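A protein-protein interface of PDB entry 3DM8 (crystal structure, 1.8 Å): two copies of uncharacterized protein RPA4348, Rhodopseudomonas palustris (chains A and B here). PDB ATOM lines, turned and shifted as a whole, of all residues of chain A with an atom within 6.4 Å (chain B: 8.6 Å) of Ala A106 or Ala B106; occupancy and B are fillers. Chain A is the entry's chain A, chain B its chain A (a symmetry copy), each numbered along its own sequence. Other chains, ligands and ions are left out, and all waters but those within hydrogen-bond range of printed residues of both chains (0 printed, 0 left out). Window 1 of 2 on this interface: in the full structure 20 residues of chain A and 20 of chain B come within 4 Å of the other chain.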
ATOM      1  N   SER A  86     -13.609 -21.653  19.509  1.00  0.00           N
ATOM      2  CA  SER A  86     -13.800 -22.623  18.470  1.00  0.00           C
ATOM      3  C   SER A  86     -15.095 -23.344  18.507  1.00  0.00           C
ATOM      4  O   SER A  86     -15.794 -23.367  19.511  1.00  0.00           O
ATOM      5  CB  SER A  86     -12.654 -23.602  18.467  1.00  0.00           C
ATOM      6  OG  SER A  86     -12.629 -24.362  19.677  1.00  0.00           O
ATOM      7  N   MET A  87     -15.407 -23.842  17.344  1.00  0.00           N
ATOM      8  CA  MET A  87     -16.598 -24.611  17.106  1.00  0.00           C
ATOM      9  C   MET A  87     -16.209 -26.018  16.719  1.00  0.00           C
ATOM     10  O   MET A  87     -15.489 -26.212  15.750  1.00  0.00           O
ATOM     11  CB  MET A  87     -17.363 -24.036  15.965  1.00  0.00           C
ATOM     12  CG  MET A  87     -18.521 -24.912  15.754  1.00  0.00           C
ATOM     13  SD  MET A  87     -19.893 -23.947  16.370  1.00  0.00           S
ATOM     14  CE  MET A  87     -20.263 -23.400  14.777  1.00  0.00           C
ATOM     15  N   VAL A  88     -16.695 -26.998  17.476  1.00  0.00           N
ATOM     16  CA  VAL A  88     -16.346 -28.385  17.239  1.00  0.00           C
ATOM     17  C   VAL A  88     -17.535 -29.293  17.448  1.00  0.00           C
ATOM     18  O   VAL A  88     -18.418 -29.005  18.253  1.00  0.00           O
ATOM     19  CB  VAL A  88     -15.174 -28.838  18.138  1.00  0.00           C
ATOM     20  CG1 VAL A  88     -14.083 -27.767  18.186  1.00  0.00           C
ATOM     21  CG2 VAL A  88     -15.637 -29.208  19.558  1.00  0.00           C
ATOM     22  N   ARG A 104     -22.720 -30.519  18.946  1.00  0.00           N
ATOM     23  CA  ARG A 104     -22.042 -29.387  18.374  1.00  0.00           C
ATOM     24  C   ARG A 104     -21.874 -28.298  19.438  1.00  0.00           C
ATOM     25  O   ARG A 104     -22.841 -27.901  20.098  1.00  0.00           O
ATOM     26  CB  ARG A 104     -22.831 -28.807  17.213  1.00  0.00           C
ATOM     27  CG  ARG A 104     -22.083 -27.704  16.620  1.00  0.00           C
ATOM     28  CD  ARG A 104     -22.780 -27.112  15.441  1.00  0.00           C
ATOM     29  NE  ARG A 104     -22.284 -27.712  14.191  1.00  0.00           N
ATOM     30  CZ  ARG A 104     -22.969 -28.563  13.446  1.00  0.00           C
ATOM     31  NH1 ARG A 104     -24.161 -29.019  13.813  1.00  0.00           N
ATOM     32  NH2 ARG A 104     -22.416 -29.022  12.345  1.00  0.00           N
ATOM     33  N   MET A 105     -20.640 -27.856  19.622  1.00  0.00           N
ATOM     34  CA  MET A 105     -20.313 -26.966  20.737  1.00  0.00           C
ATOM     35  C   MET A 105     -19.497 -25.774  20.239  1.00  0.00           C
ATOM     36  O   MET A 105     -18.761 -25.884  19.278  1.00  0.00           O
ATOM     37  CB  MET A 105     -19.520 -27.698  21.817  1.00  0.00           C
ATOM     38  CG  MET A 105     -20.087 -29.012  22.283  1.00  0.00           C
ATOM     39  SD  MET A 105     -18.837 -29.959  23.253  1.00  0.00           S
ATOM     40  CE  MET A 105     -17.672 -30.398  21.981  1.00  0.00           C
ATOM     41  N   ALA A 106     -19.657 -24.657  20.934  1.00  0.00           N
ATOM     42  CA  ALA A 106     -18.835 -23.467  20.763  1.00  0.00           C
ATOM     43  C   ALA A 106     -18.162 -23.176  22.094  1.00  0.00           C
ATOM     44  O   ALA A 106     -18.828 -23.076  23.134  1.00  0.00           O
ATOM     45  CB  ALA A 106     -19.696 -22.283  20.333  1.00  0.00           C
ATOM     46  N   LEU A 107     -16.843 -23.081  22.040  1.00  0.00           N
ATOM     47  CA  LEU A 107     -15.951 -23.011  23.209  1.00  0.00           C
ATOM     48  C   LEU A 107     -15.139 -21.707  23.168  1.00  0.00           C
ATOM     49  O   LEU A 107     -14.524 -21.392  22.169  1.00  0.00           O
ATOM     50  CB  LEU A 107     -15.005 -24.240  23.116  1.00  0.00           C
ATOM     51  CG  LEU A 107     -13.925 -24.411  24.143  1.00  0.00           C
ATOM     52  CD1 LEU A 107     -14.621 -24.811  25.445  1.00  0.00           C
ATOM     53  CD2 LEU A 107     -12.948 -25.490  23.673  1.00  0.00           C
ATOM     54  N   PHE A 108     -15.177 -20.949  24.257  1.00  0.00           N
ATOM     55  CA  PHE A 108     -14.328 -19.800  24.463  1.00  0.00           C
ATOM     56  C   PHE A 108     -13.453 -20.017  25.649  1.00  0.00           C
ATOM     57  O   PHE A 108     -13.953 -20.310  26.747  1.00  0.00           O
ATOM     58  CB  PHE A 108     -15.158 -18.523  24.673  1.00  0.00           C
ATOM     59  CG  PHE A 108     -16.034 -18.161  23.484  1.00  0.00           C
ATOM     60  CD1 PHE A 108     -17.165 -18.898  23.181  1.00  0.00           C
ATOM     61  CD2 PHE A 108     -15.699 -17.098  22.697  1.00  0.00           C
ATOM     62  CE1 PHE A 108     -17.941 -18.557  22.082  1.00  0.00           C
ATOM     63  CE2 PHE A 108     -16.466 -16.772  21.585  1.00  0.00           C
ATOM     64  CZ  PHE A 108     -17.600 -17.524  21.314  1.00  0.00           C
ATOM     65  N   ARG A 120     -16.010 -21.123  28.691  1.00  0.00           N
ATOM     66  CA  ARG A 120     -17.442 -20.987  28.471  1.00  0.00           C
ATOM     67  C   ARG A 120     -17.805 -21.803  27.252  1.00  0.00           C
ATOM     68  O   ARG A 120     -17.136 -21.740  26.207  1.00  0.00           O
ATOM     69  CB  ARG A 120     -17.840 -19.530  28.231  1.00  0.00           C
ATOM     70  CG  ARG A 120     -17.705 -18.591  29.425  1.00  0.00           C
ATOM     71  CD  ARG A 120     -18.629 -18.999  30.550  1.00  0.00           C
ATOM     72  NE  ARG A 120     -18.654 -18.028  31.633  1.00  0.00           N
ATOM     73  CZ  ARG A 120     -17.819 -18.062  32.667  1.00  0.00           C
ATOM     74  NH1 ARG A 120     -17.900 -17.179  33.619  1.00  0.00           N
ATOM     75  NH2 ARG A 120     -16.936 -19.013  32.748  1.00  0.00           N
ATOM     76  N   MET A 121     -18.791 -22.646  27.432  1.00  0.00           N
ATOM     77  CA  MET A 121     -19.289 -23.492  26.365  1.00  0.00           C
ATOM     78  C   MET A 121     -20.774 -23.366  26.180  1.00  0.00           C
ATOM     79  O   MET A 121     -21.518 -23.467  27.110  1.00  0.00           O
ATOM     80  CB  MET A 121     -18.948 -24.953  26.622  1.00  0.00           C
ATOM     81  CG  MET A 121     -19.535 -25.826  25.570  1.00  0.00           C
ATOM     82  SD  MET A 121     -19.299 -27.576  25.812  1.00  0.00           S
ATOM     83  CE  MET A 121     -17.556 -27.442  25.448  1.00  0.00           C
ATOM     84  N   VAL A 122     -21.158 -23.143  24.939  1.00  0.00           N
ATOM     85  CA  VAL A 122     -22.551 -23.179  24.451  1.00  0.00           C
ATOM     86  C   VAL A 122     -22.676 -24.334  23.499  1.00  0.00           C
ATOM     87  O   VAL A 122     -21.893 -24.488  22.572  1.00  0.00           O
ATOM     88  CB  VAL A 122     -22.898 -21.884  23.650  1.00  0.00           C
ATOM     89  CG1 VAL A 122     -24.407 -21.827  23.333  1.00  0.00           C
ATOM     90  CG2 VAL A 122     -22.496 -20.711  24.452  1.00  0.00           C
ATOM     91  N   LEU A 123     -23.707 -25.140  23.678  1.00  0.00           N
ATOM     92  CA  LEU A 123     -24.012 -26.158  22.692  1.00  0.00           C
ATOM     93  C   LEU A 123     -25.472 -26.295  22.356  1.00  0.00           C
ATOM     94  O   LEU A 123     -26.329 -25.635  22.940  1.00  0.00           O
ATOM     95  CB  LEU A 123     -23.536 -27.507  23.191  1.00  0.00           C
ATOM     96  CG  LEU A 123     -24.213 -27.951  24.462  1.00  0.00           C
ATOM     97  CD1 LEU A 123     -24.370 -29.417  24.389  1.00  0.00           C
ATOM     98  CD2 LEU A 123     -23.375 -27.536  25.660  1.00  0.00           C
ATOM     99  N   ALA B  36     -25.526 -20.380   8.749  1.00  0.00           N
ATOM    100  CA  ALA B  36     -26.323 -21.387   9.522  1.00  0.00           C
ATOM    101  C   ALA B  36     -26.535 -20.991  10.938  1.00  0.00           C
ATOM    102  O   ALA B  36     -25.620 -20.564  11.647  1.00  0.00           O
ATOM    103  CB  ALA B  36     -25.683 -22.842   9.446  1.00  0.00           C
ATOM    104  N   ILE B  37     -27.768 -21.181  11.393  1.00  0.00           N
ATOM    105  CA  ILE B  37     -28.062 -21.062  12.810  1.00  0.00           C
ATOM    106  C   ILE B  37     -28.593 -22.386  13.251  1.00  0.00           C
ATOM    107  O   ILE B  37     -29.554 -22.845  12.702  1.00  0.00           O
ATOM    108  CB  ILE B  37     -29.133 -19.993  13.146  1.00  0.00           C
ATOM    109  CG1 ILE B  37     -28.745 -18.615  12.676  1.00  0.00           C
ATOM    110  CG2 ILE B  37     -29.405 -19.964  14.689  1.00  0.00           C
ATOM    111  CD1 ILE B  37     -29.975 -17.660  12.699  1.00  0.00           C
ATOM    112  N   TYR B  38     -27.940 -23.006  14.224  1.00  0.00           N
ATOM    113  CA  TYR B  38     -28.296 -24.372  14.602  1.00  0.00           C
ATOM    114  C   TYR B  38     -29.396 -24.345  15.645  1.00  0.00           C
ATOM    115  O   TYR B  38     -29.189 -24.012  16.797  1.00  0.00           O
ATOM    116  CB  TYR B  38     -27.075 -25.158  15.109  1.00  0.00           C
ATOM    117  CG  TYR B  38     -26.037 -25.299  14.017  1.00  0.00           C
ATOM    118  CD1 TYR B  38     -24.892 -24.518  14.027  1.00  0.00           C
ATOM    119  CD2 TYR B  38     -26.233 -26.152  12.940  1.00  0.00           C
ATOM    120  CE1 TYR B  38     -23.966 -24.593  13.051  1.00  0.00           C
ATOM    121  CE2 TYR B  38     -25.273 -26.233  11.927  1.00  0.00           C
ATOM    122  CZ  TYR B  38     -24.143 -25.427  12.002  1.00  0.00           C
ATOM    123  OH  TYR B  38     -23.140 -25.444  11.053  1.00  0.00           O
ATOM    124  N   GLU B  75     -20.506 -11.016  26.130  1.00  0.00           N
ATOM    125  CA  GLU B  75     -19.770 -11.752  27.164  1.00  0.00           C
ATOM    126  C   GLU B  75     -18.335 -12.025  26.819  1.00  0.00           C
ATOM    127  O   GLU B  75     -17.462 -11.963  27.670  1.00  0.00           O
ATOM    128  CB  GLU B  75     -20.504 -13.044  27.515  1.00  0.00           C
ATOM    129  CG  GLU B  75     -21.846 -12.753  28.208  1.00  0.00           C
ATOM    130  CD  GLU B  75     -22.797 -13.985  28.398  1.00  0.00           C
ATOM    131  OE1 GLU B  75     -22.631 -15.071  27.771  1.00  0.00           O
ATOM    132  OE2 GLU B  75     -23.762 -13.841  29.170  1.00  0.00           O
ATOM    133  N   SER B  76     -18.081 -12.362  25.567  1.00  0.00           N
ATOM    134  CA  SER B  76     -16.715 -12.613  25.082  1.00  0.00           C
ATOM    135  C   SER B  76     -16.696 -12.149  23.640  1.00  0.00           C
ATOM    136  O   SER B  76     -17.671 -12.329  22.927  1.00  0.00           O
ATOM    137  CB  SER B  76     -16.342 -14.113  25.057  1.00  0.00           C
ATOM    138  OG  SER B  76     -16.838 -14.878  26.157  1.00  0.00           O
ATOM    139  N   ALA B  84     -14.403 -12.948  13.252  1.00  0.00           N
ATOM    140  CA  ALA B  84     -14.665 -12.712  14.666  1.00  0.00           C
ATOM    141  C   ALA B  84     -15.432 -13.870  15.259  1.00  0.00           C
ATOM    142  O   ALA B  84     -16.151 -14.580  14.545  1.00  0.00           O
ATOM    143  CB  ALA B  84     -15.431 -11.403  14.870  1.00  0.00           C
ATOM    144  N   ALA B  85     -15.269 -14.036  16.568  1.00  0.00           N
ATOM    145  CA  ALA B  85     -16.134 -14.942  17.360  1.00  0.00           C
ATOM    146  C   ALA B  85     -16.628 -14.215  18.584  1.00  0.00           C
ATOM    147  O   ALA B  85     -15.915 -13.407  19.197  1.00  0.00           O
ATOM    148  CB  ALA B  85     -15.368 -16.220  17.764  1.00  0.00           C
ATOM    149  N   SER B  86     -17.885 -14.430  18.918  1.00  0.00           N
ATOM    150  CA  SER B  86     -18.367 -13.843  20.135  1.00  0.00           C
ATOM    151  C   SER B  86     -19.531 -14.525  20.749  1.00  0.00           C
ATOM    152  O   SER B  86     -20.234 -15.301  20.116  1.00  0.00           O
ATOM    153  CB  SER B  86     -18.670 -12.384  19.915  1.00  0.00           C
ATOM    154  OG  SER B  86     -19.739 -12.218  18.982  1.00  0.00           O
ATOM    155  N   MET B  87     -19.633 -14.263  22.022  1.00  0.00           N
ATOM    156  CA  MET B  87     -20.688 -14.775  22.854  1.00  0.00           C
ATOM    157  C   MET B  87     -21.523 -13.622  23.358  1.00  0.00           C
ATOM    158  O   MET B  87     -21.002 -12.720  23.999  1.00  0.00           O
ATOM    159  CB  MET B  87     -20.116 -15.461  24.046  1.00  0.00           C
ATOM    160  CG  MET B  87     -21.255 -15.894  24.864  1.00  0.00           C
ATOM    161  SD  MET B  87     -21.294 -17.664  24.621  1.00  0.00           S
ATOM    162  CE  MET B  87     -20.403 -17.913  26.076  1.00  0.00           C
ATOM    163  N   VAL B  88     -22.821 -13.660  23.073  1.00  0.00           N
ATOM    164  CA  VAL B  88     -23.714 -12.583  23.454  1.00  0.00           C
ATOM    165  C   VAL B  88     -25.051 -13.116  23.914  1.00  0.00           C
ATOM    166  O   VAL B  88     -25.504 -14.166  23.461  1.00  0.00           O
ATOM    167  CB  VAL B  88     -23.917 -11.578  22.299  1.00  0.00           C
ATOM    168  CG1 VAL B  88     -22.587 -11.268  21.611  1.00  0.00           C
ATOM    169  CG2 VAL B  88     -24.959 -12.066  21.277  1.00  0.00           C
ATOM    170  N   ARG B  89     -25.641 -12.373  24.825  1.00  0.00           N
ATOM    171  CA  ARG B  89     -26.980 -12.653  25.350  1.00  0.00           C
ATOM    172  C   ARG B  89     -27.940 -11.537  24.929  1.00  0.00           C
ATOM    173  O   ARG B  89     -27.648 -10.360  25.018  1.00  0.00           O
ATOM    174  CB  ARG B  89     -26.963 -12.759  26.853  1.00  0.00           C
ATOM    175  CG  ARG B  89     -27.719 -13.951  27.352  1.00  0.00           C
ATOM    176  CD  ARG B  89     -28.217 -13.771  28.723  1.00  0.00           C
ATOM    177  NE  ARG B  89     -27.464 -12.772  29.453  1.00  0.00           N
ATOM    178  CZ  ARG B  89     -28.062 -11.905  30.256  1.00  0.00           C
ATOM    179  NH1 ARG B  89     -29.384 -11.956  30.376  1.00  0.00           N
ATOM    180  NH2 ARG B  89     -27.357 -11.007  30.933  1.00  0.00           N
ATOM    181  N   VAL B 103     -31.771 -15.218  25.338  1.00  0.00           N
ATOM    182  CA  VAL B 103     -31.099 -16.136  24.410  1.00  0.00           C
ATOM    183  C   VAL B 103     -29.600 -15.945  24.501  1.00  0.00           C
ATOM    184  O   VAL B 103     -29.122 -14.839  24.317  1.00  0.00           O
ATOM    185  CB  VAL B 103     -31.542 -15.858  22.965  1.00  0.00           C
ATOM    186  CG1 VAL B 103     -30.953 -16.880  22.018  1.00  0.00           C
ATOM    187  CG2 VAL B 103     -33.075 -15.894  22.865  1.00  0.00           C
ATOM    188  N   ARG B 104     -28.869 -17.024  24.797  1.00  0.00           N
ATOM    189  CA  ARG B 104     -27.433 -16.951  24.810  1.00  0.00           C
ATOM    190  C   ARG B 104     -26.873 -17.625  23.553  1.00  0.00           C
ATOM    191  O   ARG B 104     -27.218 -18.771  23.240  1.00  0.00           O
ATOM    192  CB  ARG B 104     -26.861 -17.655  26.028  1.00  0.00           C
ATOM    193  CG  ARG B 104     -25.409 -17.504  26.039  1.00  0.00           C
ATOM    194  CD  ARG B 104     -24.780 -18.134  27.237  1.00  0.00           C
ATOM    195  NE  ARG B 104     -24.582 -17.139  28.302  1.00  0.00           N
ATOM    196  CZ  ARG B 104     -25.292 -17.083  29.417  1.00  0.00           C
ATOM    197  NH1 ARG B 104     -26.320 -17.893  29.637  1.00  0.00           N
ATOM    198  NH2 ARG B 104     -25.010 -16.148  30.297  1.00  0.00           N
ATOM    199  N   MET B 105     -26.046 -16.892  22.824  1.00  0.00           N
ATOM    200  CA  MET B 105     -25.600 -17.341  21.504  1.00  0.00           C
ATOM    201  C   MET B 105     -24.083 -17.201  21.385  1.00  0.00           C
ATOM    202  O   MET B 105     -23.490 -16.333  21.995  1.00  0.00           O
ATOM    203  CB  MET B 105     -26.264 -16.535  20.390  1.00  0.00           C
ATOM    204  CG  MET B 105     -27.761 -16.399  20.471  1.00  0.00           C
ATOM    205  SD  MET B 105     -28.361 -15.081  19.328  1.00  0.00           S
ATOM    206  CE  MET B 105     -27.733 -13.619  20.126  1.00  0.00           C
ATOM    207  N   ALA B 106     -23.502 -18.080  20.579  1.00  0.00           N
ATOM    208  CA  ALA B 106     -22.109 -18.005  20.164  1.00  0.00           C
ATOM    209  C   ALA B 106     -22.084 -17.898  18.648  1.00  0.00           C
ATOM    210  O   ALA B 106     -22.685 -18.721  17.943  1.00  0.00           O
ATOM    211  CB  ALA B 106     -21.351 -19.248  20.622  1.00  0.00           C
ATOM    212  N   LEU B 107     -21.414 -16.859  18.176  1.00  0.00           N
ATOM    213  CA  LEU B 107     -21.413 -16.420  16.771  1.00  0.00           C
ATOM    214  C   LEU B 107     -19.980 -16.443  16.218  1.00  0.00           C
ATOM    215  O   LEU B 107     -19.076 -15.892  16.816  1.00  0.00           O
ATOM    216  CB  LEU B 107     -21.973 -14.970  16.762  1.00  0.00           C
ATOM    217  CG  LEU B 107     -22.034 -14.218  15.466  1.00  0.00           C
ATOM    218  CD1 LEU B 107     -23.156 -14.856  14.644  1.00  0.00           C
ATOM    219  CD2 LEU B 107     -22.315 -12.742  15.751  1.00  0.00           C
ATOM    220  N   PHE B 108     -19.789 -17.115  15.089  1.00  0.00           N
ATOM    221  CA  PHE B 108     -18.561 -17.078  14.333  1.00  0.00           C
ATOM    222  C   PHE B 108     -18.808 -16.503  12.981  1.00  0.00           C
ATOM    223  O   PHE B 108     -19.681 -16.993  12.246  1.00  0.00           O
ATOM    224  CB  PHE B 108     -17.956 -18.483  14.183  1.00  0.00           C
ATOM    225  CG  PHE B 108     -17.588 -19.136  15.506  1.00  0.00           C
ATOM    226  CD1 PHE B 108     -18.567 -19.601  16.367  1.00  0.00           C
ATOM    227  CD2 PHE B 108     -16.276 -19.259  15.857  1.00  0.00           C
ATOM    228  CE1 PHE B 108     -18.207 -20.180  17.577  1.00  0.00           C
ATOM    229  CE2 PHE B 108     -15.920 -19.819  17.079  1.00  0.00           C
ATOM    230  CZ  PHE B 108     -16.923 -20.287  17.914  1.00  0.00           C
ATOM    231  N   THR B 109     -18.052 -15.445  12.646  1.00  0.00           N
ATOM    232  CA  THR B 109     -18.265 -14.723  11.407  1.00  0.00           C
ATOM    233  C   THR B 109     -16.972 -14.553  10.607  1.00  0.00           C
ATOM    234  O   THR B 109     -15.888 -14.449  11.149  1.00  0.00           O
ATOM    235  CB  THR B 109     -18.821 -13.295  11.692  1.00  0.00           C
ATOM    236  OG1 THR B 109     -18.015 -12.685  12.660  1.00  0.00           O
ATOM    237  CG2 THR B 109     -20.200 -13.348  12.293  1.00  0.00           C
ATOM    238  N   LEU B 119     -21.454 -17.087   8.361  1.00  0.00           N
ATOM    239  CA  LEU B 119     -21.933 -17.030   9.721  1.00  0.00           C
ATOM    240  C   LEU B 119     -22.380 -18.374  10.220  1.00  0.00           C
ATOM    241  O   LEU B 119     -23.051 -19.151   9.496  1.00  0.00           O
ATOM    242  CB  LEU B 119     -23.084 -16.000   9.830  1.00  0.00           C
ATOM    243  CG  LEU B 119     -23.723 -15.803  11.196  1.00  0.00           C
ATOM    244  CD1 LEU B 119     -24.181 -14.331  11.374  1.00  0.00           C
ATOM    245  CD2 LEU B 119     -24.948 -16.772  11.522  1.00  0.00           C
ATOM    246  N   ARG B 120     -21.974 -18.661  11.453  1.00  0.00           N
ATOM    247  CA  ARG B 120     -22.400 -19.857  12.165  1.00  0.00           C
ATOM    248  C   ARG B 120     -22.762 -19.455  13.576  1.00  0.00           C
ATOM    249  O   ARG B 120     -22.025 -18.715  14.248  1.00  0.00           O
ATOM    250  CB  ARG B 120     -21.290 -20.908  12.216  1.00  0.00           C
ATOM    251  CG  ARG B 120     -20.917 -21.557  10.888  1.00  0.00           C
ATOM    252  CD  ARG B 120     -22.078 -22.338  10.314  1.00  0.00           C
ATOM    253  NE  ARG B 120     -21.706 -23.111   9.139  1.00  0.00           N
ATOM    254  CZ  ARG B 120     -21.763 -22.634   7.899  1.00  0.00           C
ATOM    255  NH1 ARG B 120     -21.437 -23.377   6.883  1.00  0.00           N
ATOM    256  NH2 ARG B 120     -22.189 -21.422   7.698  1.00  0.00           N
ATOM    257  N   MET B 121     -23.947 -19.850  13.970  1.00  0.00           N
ATOM    258  CA  MET B 121     -24.450 -19.575  15.302  1.00  0.00           C
ATOM    259  C   MET B 121     -24.921 -20.816  16.004  1.00  0.00           C
ATOM    260  O   MET B 121     -25.678 -21.571  15.471  1.00  0.00           O
ATOM    261  CB  MET B 121     -25.594 -18.571  15.257  1.00  0.00           C
ATOM    262  CG  MET B 121     -26.163 -18.358  16.615  1.00  0.00           C
ATOM    263  SD  MET B 121     -27.584 -17.284  16.686  1.00  0.00           S
ATOM    264  CE  MET B 121     -26.581 -15.851  16.323  1.00  0.00           C
ATOM    265  N   VAL B 122     -24.434 -20.980  17.218  1.00  0.00           N
ATOM    266  CA  VAL B 122     -24.882 -21.995  18.193  1.00  0.00           C
ATOM    267  C   VAL B 122     -25.520 -21.274  19.347  1.00  0.00           C
ATOM    268  O   VAL B 122     -24.955 -20.351  19.916  1.00  0.00           O
ATOM    269  CB  VAL B 122     -23.670 -22.796  18.765  1.00  0.00           C
ATOM    270  CG1 VAL B 122     -24.157 -23.992  19.610  1.00  0.00           C
ATOM    271  CG2 VAL B 122     -22.841 -23.267  17.637  1.00  0.00           C
ATOM    272  N   LEU B 123     -26.693 -21.726  19.750  1.00  0.00           N
ATOM    273  CA  LEU B 123     -27.284 -21.219  20.973  1.00  0.00           C
ATOM    274  C   LEU B 123     -27.901 -22.266  21.859  1.00  0.00           C
ATOM    275  O   LEU B 123     -27.954 -23.446  21.516  1.00  0.00           O
ATOM    276  CB  LEU B 123     -28.369 -20.217  20.636  1.00  0.00           C
ATOM    277  CG  LEU B 123     -29.508 -20.809  19.846  1.00  0.00           C
ATOM    278  CD1 LEU B 123     -30.747 -20.140  20.288  1.00  0.00           C
ATOM    279  CD2 LEU B 123     -29.260 -20.604  18.360  1.00  0.00           C
ATOM    280  N   ASP B 124     -28.203 -21.822  23.069  1.00  0.00           N
ATOM    281  CA  ASP B 124     -28.766 -22.721  24.125  1.00  0.00           C
ATOM    282  C   ASP B 124     -30.238 -22.915  23.782  1.00  0.00           C
ATOM    283  O   ASP B 124     -31.150 -22.227  24.251  1.00  0.00           O
ATOM    284  CB  ASP B 124     -28.468 -22.189  25.553  1.00  0.00           C
ATOM    285  CG  ASP B 124     -28.913 -23.177  26.658  1.00  0.00           C
ATOM    286  OD1 ASP B 124     -29.626 -24.167  26.343  1.00  0.00           O
ATOM    287  OD2 ASP B 124     -28.668 -22.910  27.856  1.00  0.00           O
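Along chain B the printed residues that touch a printed residue of chain A span positions 38 to 124. Of the 12 printed residues of chain A, 8 touch a printed residue of chain B. Hydrophobic or aromatic side chains of chain A that line the printed part of chain B: Met A87, Ala A106, Phe A108 and Val A122.
Met A87 touches Phe B108, and with the chains exchanged Phe A108 touches Met B87. Met A87 touches Arg B120, and with the chains exchanged Arg A120 touches Met B87. Met A87 touches Val B122, and with the chains exchanged Val A122 touches Met B87. Val A122 touches its own counterpart, Val B122. Positions printed for both chains: 86, 87, 88, 104, 105, 106, 107, 108, 120, 121, 122 and 123. Of the 20 pairs that touch across the chains among the printed residues, 15 have their exchanged pair printed and touching as well.
Met A87 touches Phe B108 (N to CZ, 3.9 Å). Met A87 touches Arg B120. Tyr B38 touches Arg A104 (CE2 to NH1, 3.5 Å). Phe A108 touches Ala B85. Phe A108 touches Met B87 (CZ to N, 3.9 Å). Val A122 touches Met B87 (CG2 to SD, 3.3 Å). Val A122 touches Val B122 (O to CG1, 3.8 Å). Val A122 touches Leu B123. Val A122 touches Asp B124. Val B122 touches Leu A123.
Of the printed residues of chain B, Arg A104 touches Tyr B38 (3.5 Å). Of chain B, only Ala B106 and Phe B108 come within 4 Å of Ala A106. Of the printed residues of chain A, Tyr B38 touches Arg A104 (3.5 Å). Of the printed residues of chain A, Ser B86 touches Phe A108 (3.6 Å). Val B103 touches none of the printed residues of chain A. Of chain A, only Ala A106 and Phe A108 come within 4 Å of Ala B106. Leu B119 touches none of the printed residues of chain A. Of the printed residues of chain A, Leu B123 touches Val A122 and Leu A123. Of the printed residues of chain A, Asp B124 touches Val A122 (3.8 Å) and Leu A123 (3.98 Å). The nearest residue of chain B that does not touch Ala A106 is Val B122 (4.3 Å). The nearest printed residue of chain A that does not touch Val B122 is Arg A104 (4.2 Å).
The backbone carbonyl oxygen of Leu A123 lies close to the backbone carbonyl oxygen of Leu B123, at 3.1 Å.
The backbone NH of Tyr B38 sits at hydrogen-bond distance from the backbone carbonyl oxygen of Met B121 (3.0 Å). The backbone carbonyl oxygen (O) of Ser B86 is in hydrogen-bond range of the backbone NH (N) of Leu B107 (2.8 Å). O of Ser B76 sits at hydrogen-bond distance from N of Met B87 (2.9 Å). The backbone carbonyl oxygen (O) of Val A122 sits at hydrogen-bond distance from the backbone NH (N) of Ala A106 (2.8 Å). O of Arg B120 is in hydrogen-bond range of N of Phe B108, 2.9 Å away. The side-chain hydroxyl (OH) of Tyr B38 lies within hydrogen-bond range of the guanidinium group (NE) of Arg B120, 3.3 Å away.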
